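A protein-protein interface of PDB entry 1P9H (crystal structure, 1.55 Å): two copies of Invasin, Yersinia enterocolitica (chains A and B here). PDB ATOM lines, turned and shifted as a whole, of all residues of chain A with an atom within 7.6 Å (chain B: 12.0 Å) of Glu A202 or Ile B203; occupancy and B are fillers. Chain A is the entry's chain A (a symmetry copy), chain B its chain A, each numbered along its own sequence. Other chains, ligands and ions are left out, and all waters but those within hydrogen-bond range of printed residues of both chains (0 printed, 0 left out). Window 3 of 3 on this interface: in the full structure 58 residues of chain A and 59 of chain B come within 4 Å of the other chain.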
ATOM      1  N   GLY A 187     -35.075 -17.387  16.522  1.00  0.00           N
ATOM      2  CA  GLY A 187     -36.267 -18.162  16.806  1.00  0.00           C
ATOM      3  C   GLY A 187     -36.050 -19.119  17.964  1.00  0.00           C
ATOM      4  O   GLY A 187     -34.921 -19.537  18.232  1.00  0.00           O
ATOM      5  N   VAL A 194     -35.375 -18.444  11.612  1.00  0.00           N
ATOM      6  CA  VAL A 194     -33.987 -18.519  12.061  1.00  0.00           C
ATOM      7  C   VAL A 194     -33.172 -17.375  11.463  1.00  0.00           C
ATOM      8  O   VAL A 194     -33.347 -17.044  10.291  1.00  0.00           O
ATOM      9  CB  VAL A 194     -33.350 -19.868  11.618  1.00  0.00           C
ATOM     10  CG1 VAL A 194     -31.844 -19.845  11.842  1.00  0.00           C
ATOM     11  CG2 VAL A 194     -33.980 -21.014  12.390  1.00  0.00           C
ATOM     12  N   VAL A 196     -29.219 -15.392  10.830  1.00  0.00           N
ATOM     13  CA  VAL A 196     -27.850 -15.778  10.506  1.00  0.00           C
ATOM     14  C   VAL A 196     -27.009 -16.188  11.715  1.00  0.00           C
ATOM     15  O   VAL A 196     -26.346 -17.229  11.686  1.00  0.00           O
ATOM     16  CB  VAL A 196     -27.134 -14.643   9.735  1.00  0.00           C
ATOM     17  CG1 VAL A 196     -25.654 -14.968   9.563  1.00  0.00           C
ATOM     18  CG2 VAL A 196     -27.787 -14.462   8.365  1.00  0.00           C
ATOM     19  N   ALA A 197     -27.039 -15.381  12.770  1.00  0.00           N
ATOM     20  CA  ALA A 197     -26.270 -15.675  13.979  1.00  0.00           C
ATOM     21  C   ALA A 197     -26.637 -17.046  14.538  1.00  0.00           C
ATOM     22  O   ALA A 197     -25.776 -17.799  15.000  1.00  0.00           O
ATOM     23  CB  ALA A 197     -26.527 -14.604  15.031  1.00  0.00           C
ATOM     24  N   GLN A 198     -27.927 -17.351  14.493  1.00  0.00           N
ATOM     25  CA  GLN A 198     -28.457 -18.614  14.988  1.00  0.00           C
ATOM     26  C   GLN A 198     -27.967 -19.785  14.139  1.00  0.00           C
ATOM     27  O   GLN A 198     -27.600 -20.837  14.666  1.00  0.00           O
ATOM     28  CB  GLN A 198     -29.983 -18.530  14.981  1.00  0.00           C
ATOM     29  CG  GLN A 198     -30.723 -19.774  15.401  1.00  0.00           C
ATOM     30  CD  GLN A 198     -32.173 -19.467  15.710  1.00  0.00           C
ATOM     31  OE1 GLN A 198     -32.789 -18.617  15.061  1.00  0.00           O
ATOM     32  NE2 GLN A 198     -32.728 -20.156  16.697  1.00  0.00           N
ATOM     33  N   LEU A 199     -27.959 -19.597  12.824  1.00  0.00           N
ATOM     34  CA  LEU A 199     -27.497 -20.631  11.907  1.00  0.00           C
ATOM     35  C   LEU A 199     -26.042 -20.964  12.219  1.00  0.00           C
ATOM     36  O   LEU A 199     -25.680 -22.128  12.378  1.00  0.00           O
ATOM     37  CB  LEU A 199     -27.614 -20.143  10.461  1.00  0.00           C
ATOM     38  CG  LEU A 199     -27.014 -21.032   9.368  1.00  0.00           C
ATOM     39  CD1 LEU A 199     -27.709 -22.383   9.347  1.00  0.00           C
ATOM     40  CD2 LEU A 199     -27.159 -20.341   8.020  1.00  0.00           C
ATOM     41  N   LYS A 200     -25.215 -19.927  12.313  1.00  0.00           N
ATOM     42  CA  LYS A 200     -23.796 -20.101  12.602  1.00  0.00           C
ATOM     43  C   LYS A 200     -23.568 -20.782  13.948  1.00  0.00           C
ATOM     44  O   LYS A 200     -22.789 -21.732  14.049  1.00  0.00           O
ATOM     45  CB  LYS A 200     -23.089 -18.744  12.585  1.00  0.00           C
ATOM     46  CG  LYS A 200     -23.108 -18.060  11.226  1.00  0.00           C
ATOM     47  CD  LYS A 200     -22.407 -16.714  11.270  1.00  0.00           C
ATOM     48  CE  LYS A 200     -22.360 -16.073   9.892  1.00  0.00           C
ATOM     49  NZ  LYS A 200     -21.652 -14.764   9.912  1.00  0.00           N
ATOM     50  N   LYS A 201     -24.251 -20.294  14.979  1.00  0.00           N
ATOM     51  CA  LYS A 201     -24.119 -20.851  16.319  1.00  0.00           C
ATOM     52  C   LYS A 201     -24.424 -22.345  16.350  1.00  0.00           C
ATOM     53  O   LYS A 201     -23.599 -23.146  16.794  1.00  0.00           O
ATOM     54  CB  LYS A 201     -25.039 -20.109  17.282  1.00  0.00           C
ATOM     55  N   GLU A 202     -25.610 -22.720  15.878  1.00  0.00           N
ATOM     56  CA  GLU A 202     -26.014 -24.120  15.865  1.00  0.00           C
ATOM     57  C   GLU A 202     -25.016 -25.006  15.129  1.00  0.00           C
ATOM     58  O   GLU A 202     -24.709 -26.110  15.578  1.00  0.00           O
ATOM     59  CB  GLU A 202     -27.401 -24.269  15.232  1.00  0.00           C
ATOM     60  CG  GLU A 202     -28.522 -23.625  16.034  1.00  0.00           C
ATOM     61  CD  GLU A 202     -28.629 -24.180  17.443  1.00  0.00           C
ATOM     62  OE1 GLU A 202     -27.688 -23.978  18.241  1.00  0.00           O
ATOM     63  OE2 GLU A 202     -29.655 -24.820  17.756  1.00  0.00           O
ATOM     64  N   ILE A 203     -24.510 -24.521  13.999  1.00  0.00           N
ATOM     65  CA  ILE A 203     -23.542 -25.283  13.220  1.00  0.00           C
ATOM     66  C   ILE A 203     -22.247 -25.464  14.003  1.00  0.00           C
ATOM     67  O   ILE A 203     -21.734 -26.577  14.125  1.00  0.00           O
ATOM     68  CB  ILE A 203     -23.218 -24.583  11.881  1.00  0.00           C
ATOM     69  CG1 ILE A 203     -24.466 -24.545  10.997  1.00  0.00           C
ATOM     70  CG2 ILE A 203     -22.089 -25.317  11.169  1.00  0.00           C
ATOM     71  CD1 ILE A 203     -24.249 -23.880   9.655  1.00  0.00           C
ATOM     72  N   GLU A 204     -21.722 -24.363  14.536  1.00  0.00           N
ATOM     73  CA  GLU A 204     -20.486 -24.396  15.308  1.00  0.00           C
ATOM     74  C   GLU A 204     -20.529 -25.508  16.351  1.00  0.00           C
ATOM     75  O   GLU A 204     -19.566 -26.257  16.514  1.00  0.00           O
ATOM     76  CB  GLU A 204     -20.257 -23.051  15.985  1.00  0.00           C
ATOM     77  N   LYS A 205     -21.651 -25.611  17.056  1.00  0.00           N
ATOM     78  CA  LYS A 205     -21.812 -26.638  18.077  1.00  0.00           C
ATOM     79  C   LYS A 205     -22.442 -27.898  17.486  1.00  0.00           C
ATOM     80  O   LYS A 205     -23.533 -28.294  17.948  1.00  0.00           O
ATOM     81  CB  LYS A 205     -22.673 -26.110  19.229  1.00  0.00           C
ATOM     82  CG  LYS A 205     -24.036 -25.586  18.807  1.00  0.00           C
ATOM     83  CD  LYS A 205     -24.845 -25.107  20.004  1.00  0.00           C
ATOM     84  CE  LYS A 205     -24.153 -23.957  20.722  1.00  0.00           C
ATOM     85  NZ  LYS A 205     -24.958 -23.454  21.872  1.00  0.00           N
ATOM     86  N   VAL B 194     -36.295 -20.369   6.495  1.00  0.00           N
ATOM     87  CA  VAL B 194     -36.067 -21.590   7.265  1.00  0.00           C
ATOM     88  C   VAL B 194     -36.549 -21.409   8.703  1.00  0.00           C
ATOM     89  O   VAL B 194     -36.342 -20.348   9.291  1.00  0.00           O
ATOM     90  CB  VAL B 194     -34.550 -21.935   7.289  1.00  0.00           C
ATOM     91  CG1 VAL B 194     -34.270 -23.039   8.299  1.00  0.00           C
ATOM     92  CG2 VAL B 194     -34.096 -22.362   5.903  1.00  0.00           C
ATOM     93  N   ASN B 195     -37.205 -22.425   9.268  1.00  0.00           N
ATOM     94  CA  ASN B 195     -37.640 -22.317  10.657  1.00  0.00           C
ATOM     95  C   ASN B 195     -36.716 -23.129  11.559  1.00  0.00           C
ATOM     96  O   ASN B 195     -35.846 -23.851  11.072  1.00  0.00           O
ATOM     97  CB  ASN B 195     -39.117 -22.726  10.850  1.00  0.00           C
ATOM     98  CG  ASN B 195     -39.392 -24.193  10.554  1.00  0.00           C
ATOM     99  OD1 ASN B 195     -38.507 -25.045  10.631  1.00  0.00           O
ATOM    100  ND2 ASN B 195     -40.650 -24.493  10.240  1.00  0.00           N
ATOM    101  N   VAL B 196     -36.891 -22.988  12.868  1.00  0.00           N
ATOM    102  CA  VAL B 196     -36.051 -23.679  13.840  1.00  0.00           C
ATOM    103  C   VAL B 196     -36.029 -25.199  13.684  1.00  0.00           C
ATOM    104  O   VAL B 196     -34.956 -25.808  13.680  1.00  0.00           O
ATOM    105  CB  VAL B 196     -36.472 -23.309  15.282  1.00  0.00           C
ATOM    106  CG1 VAL B 196     -35.724 -24.171  16.293  1.00  0.00           C
ATOM    107  CG2 VAL B 196     -36.177 -21.832  15.540  1.00  0.00           C
ATOM    108  N   ALA B 197     -37.204 -25.807  13.553  1.00  0.00           N
ATOM    109  CA  ALA B 197     -37.300 -27.259  13.401  1.00  0.00           C
ATOM    110  C   ALA B 197     -36.489 -27.736  12.202  1.00  0.00           C
ATOM    111  O   ALA B 197     -35.830 -28.778  12.249  1.00  0.00           O
ATOM    112  CB  ALA B 197     -38.758 -27.668  13.233  1.00  0.00           C
ATOM    113  N   GLN B 198     -36.553 -26.961  11.127  1.00  0.00           N
ATOM    114  CA  GLN B 198     -35.846 -27.265   9.891  1.00  0.00           C
ATOM    115  C   GLN B 198     -34.334 -27.176  10.086  1.00  0.00           C
ATOM    116  O   GLN B 198     -33.583 -28.021   9.594  1.00  0.00           O
ATOM    117  CB  GLN B 198     -36.321 -26.290   8.814  1.00  0.00           C
ATOM    118  CG  GLN B 198     -35.654 -26.404   7.468  1.00  0.00           C
ATOM    119  CD  GLN B 198     -36.441 -25.667   6.405  1.00  0.00           C
ATOM    120  OE1 GLN B 198     -37.031 -24.616   6.673  1.00  0.00           O
ATOM    121  NE2 GLN B 198     -36.454 -26.208   5.195  1.00  0.00           N
ATOM    122  N   LEU B 199     -33.893 -26.151  10.807  1.00  0.00           N
ATOM    123  CA  LEU B 199     -32.474 -25.965  11.079  1.00  0.00           C
ATOM    124  C   LEU B 199     -31.946 -27.177  11.839  1.00  0.00           C
ATOM    125  O   LEU B 199     -30.932 -27.765  11.465  1.00  0.00           O
ATOM    126  CB  LEU B 199     -32.260 -24.701  11.917  1.00  0.00           C
ATOM    127  CG  LEU B 199     -30.847 -24.438  12.445  1.00  0.00           C
ATOM    128  CD1 LEU B 199     -29.875 -24.270  11.289  1.00  0.00           C
ATOM    129  CD2 LEU B 199     -30.859 -23.189  13.314  1.00  0.00           C
ATOM    130  N   LYS B 200     -32.648 -27.548  12.905  1.00  0.00           N
ATOM    131  CA  LYS B 200     -32.255 -28.687  13.725  1.00  0.00           C
ATOM    132  C   LYS B 200     -32.228 -29.986  12.923  1.00  0.00           C
ATOM    133  O   LYS B 200     -31.261 -30.746  12.986  1.00  0.00           O
ATOM    134  CB  LYS B 200     -33.211 -28.834  14.911  1.00  0.00           C
ATOM    135  CG  LYS B 200     -33.178 -27.656  15.874  1.00  0.00           C
ATOM    136  CD  LYS B 200     -34.154 -27.847  17.021  1.00  0.00           C
ATOM    137  CE  LYS B 200     -34.058 -26.705  18.019  1.00  0.00           C
ATOM    138  NZ  LYS B 200     -34.990 -26.889  19.166  1.00  0.00           N
ATOM    139  N   LYS B 201     -33.294 -30.233  12.169  1.00  0.00           N
ATOM    140  CA  LYS B 201     -33.398 -31.441  11.360  1.00  0.00           C
ATOM    141  C   LYS B 201     -32.224 -31.585  10.396  1.00  0.00           C
ATOM    142  O   LYS B 201     -31.527 -32.601  10.403  1.00  0.00           O
ATOM    143  CB  LYS B 201     -34.712 -31.438  10.587  1.00  0.00           C
ATOM    144  N   GLU B 202     -32.007 -30.568   9.567  1.00  0.00           N
ATOM    145  CA  GLU B 202     -30.919 -30.597   8.597  1.00  0.00           C
ATOM    146  C   GLU B 202     -29.565 -30.850   9.251  1.00  0.00           C
ATOM    147  O   GLU B 202     -28.751 -31.610   8.726  1.00  0.00           O
ATOM    148  CB  GLU B 202     -30.874 -29.285   7.808  1.00  0.00           C
ATOM    149  CG  GLU B 202     -32.085 -29.056   6.915  1.00  0.00           C
ATOM    150  CD  GLU B 202     -32.284 -30.166   5.899  1.00  0.00           C
ATOM    151  OE1 GLU B 202     -32.568 -31.311   6.309  1.00  0.00           O
ATOM    152  OE2 GLU B 202     -32.156 -29.894   4.686  1.00  0.00           O
ATOM    153  N   ILE B 203     -29.327 -30.214  10.393  1.00  0.00           N
ATOM    154  CA  ILE B 203     -28.068 -30.391  11.104  1.00  0.00           C
ATOM    155  C   ILE B 203     -27.926 -31.827  11.596  1.00  0.00           C
ATOM    156  O   ILE B 203     -26.899 -32.470  11.374  1.00  0.00           O
ATOM    157  CB  ILE B 203     -27.965 -29.439  12.318  1.00  0.00           C
ATOM    158  CG1 ILE B 203     -27.927 -27.987  11.838  1.00  0.00           C
ATOM    159  CG2 ILE B 203     -26.716 -29.761  13.129  1.00  0.00           C
ATOM    160  CD1 ILE B 203     -27.823 -26.973  12.958  1.00  0.00           C
ATOM    161  N   GLU B 204     -28.963 -32.326  12.263  1.00  0.00           N
ATOM    162  CA  GLU B 204     -28.957 -33.686  12.788  1.00  0.00           C
ATOM    163  C   GLU B 204     -28.501 -34.676  11.722  1.00  0.00           C
ATOM    164  O   GLU B 204     -27.683 -35.556  11.989  1.00  0.00           O
ATOM    165  CB  GLU B 204     -30.348 -34.058  13.287  1.00  0.00           C
ATOM    166  N   LYS B 205     -29.033 -34.528  10.513  1.00  0.00           N
ATOM    167  CA  LYS B 205     -28.669 -35.410   9.412  1.00  0.00           C
ATOM    168  C   LYS B 205     -27.497 -34.834   8.619  1.00  0.00           C
ATOM    169  O   LYS B 205     -27.662 -34.583   7.406  1.00  0.00           O
ATOM    170  CB  LYS B 205     -29.872 -35.630   8.489  1.00  0.00           C
ATOM    171  CG  LYS B 205     -30.487 -34.352   7.942  1.00  0.00           C
ATOM    172  CD  LYS B 205     -31.656 -34.649   7.013  1.00  0.00           C
ATOM    173  CE  LYS B 205     -32.775 -35.382   7.737  1.00  0.00           C
ATOM    174  NZ  LYS B 205     -33.941 -35.641   6.845  1.00  0.00           N
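The backbone NH of Ala B197 lies within hydrogen-bond range of the side-chain amide oxygen of Asn B195, 3.3 Å away. OD1 of Asn B195 is in hydrogen-bond range of N of Gln B198 (2.8 Å). O of Gly A187 is in hydrogen-bond range of NE2 of Gln A198, at 2.7 Å.
Of the printed residues of chain B, Gly A187 touches Val B196. Printed residues of chain B within 4 Å of Val A194: Val B194 (3.2 Å), Asn B195 (3.6 Å), Val B196 (3.5 Å) and Leu B199 (3.8 Å). Val A196 touches none of the printed residues of chain B. Gln A198 touches none of the printed residues of chain B. Glu A202 touches just these residues of chain B: Leu B199 (3.6 Å) and Ile B203 (3.6 Å). No residue of chain B comes within 4 Å of Ile A203. No residue of chain B comes within 4 Å of Glu A204. No residue of chain B comes within 4 Å of Lys A205. Printed residues of chain A within 4 Å of Asn B195: Val A194. Ile B203 touches one residue of chain A. The nearest residue of chain B that does not touch Glu A202 is Lys B200 (4.8 Å).
Val A194 touches its own counterpart, Val B194. Val A194 touches Val B196, but with the chains exchanged Val A196 does not touch Val B194 (8.8 Å). Glu A202 touches Leu B199, but with the chains exchanged Leu A199 does not touch Glu B202 (7.7 Å). Glu A202 touches Ile B203, but with the chains exchanged Ile A203 does not touch Glu B202 (8.3 Å). Positions printed for both chains: 194, 196, 197, 198, 199, 200, 201, 202, 203, 204 and 205. Of the 8 pairs that touch across the chains among the printed residues, 2 have their exchanged pair printed and touching as well.
Printed residues of chain B that touch a printed residue of chain A: Val B194, Asn B195, Val B196, Leu B199 and Ile B203. Hydrophobic or aromatic side chains of chain B within 4 Å of the printed part of chain A: Val B196, Leu B199 and Ile B203. Printed residues of chain A that touch a printed residue of chain B: Gly A187, Val A194, Leu A199 and Glu A202. Hydrophobic or aromatic side chains of chain A within 4 Å of the printed part of chain B: Val A194 and Leu A199.
The backbone carbonyl oxygen of Val B194 lies within hydrogen-bond range of the backbone NH of Val A194.
Val B196 touches Gly A187 (CG2 to C, 3.6 Å). Asn B195 touches Val A194 (C to CG2, 3.6 Å). Val B196 touches Val A194. Val A194 touches Leu B199. Leu A199 touches Leu B199. Glu A202 touches Leu B199 (CG to CD2, 3.6 Å). Glu A202 touches Ile B203.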
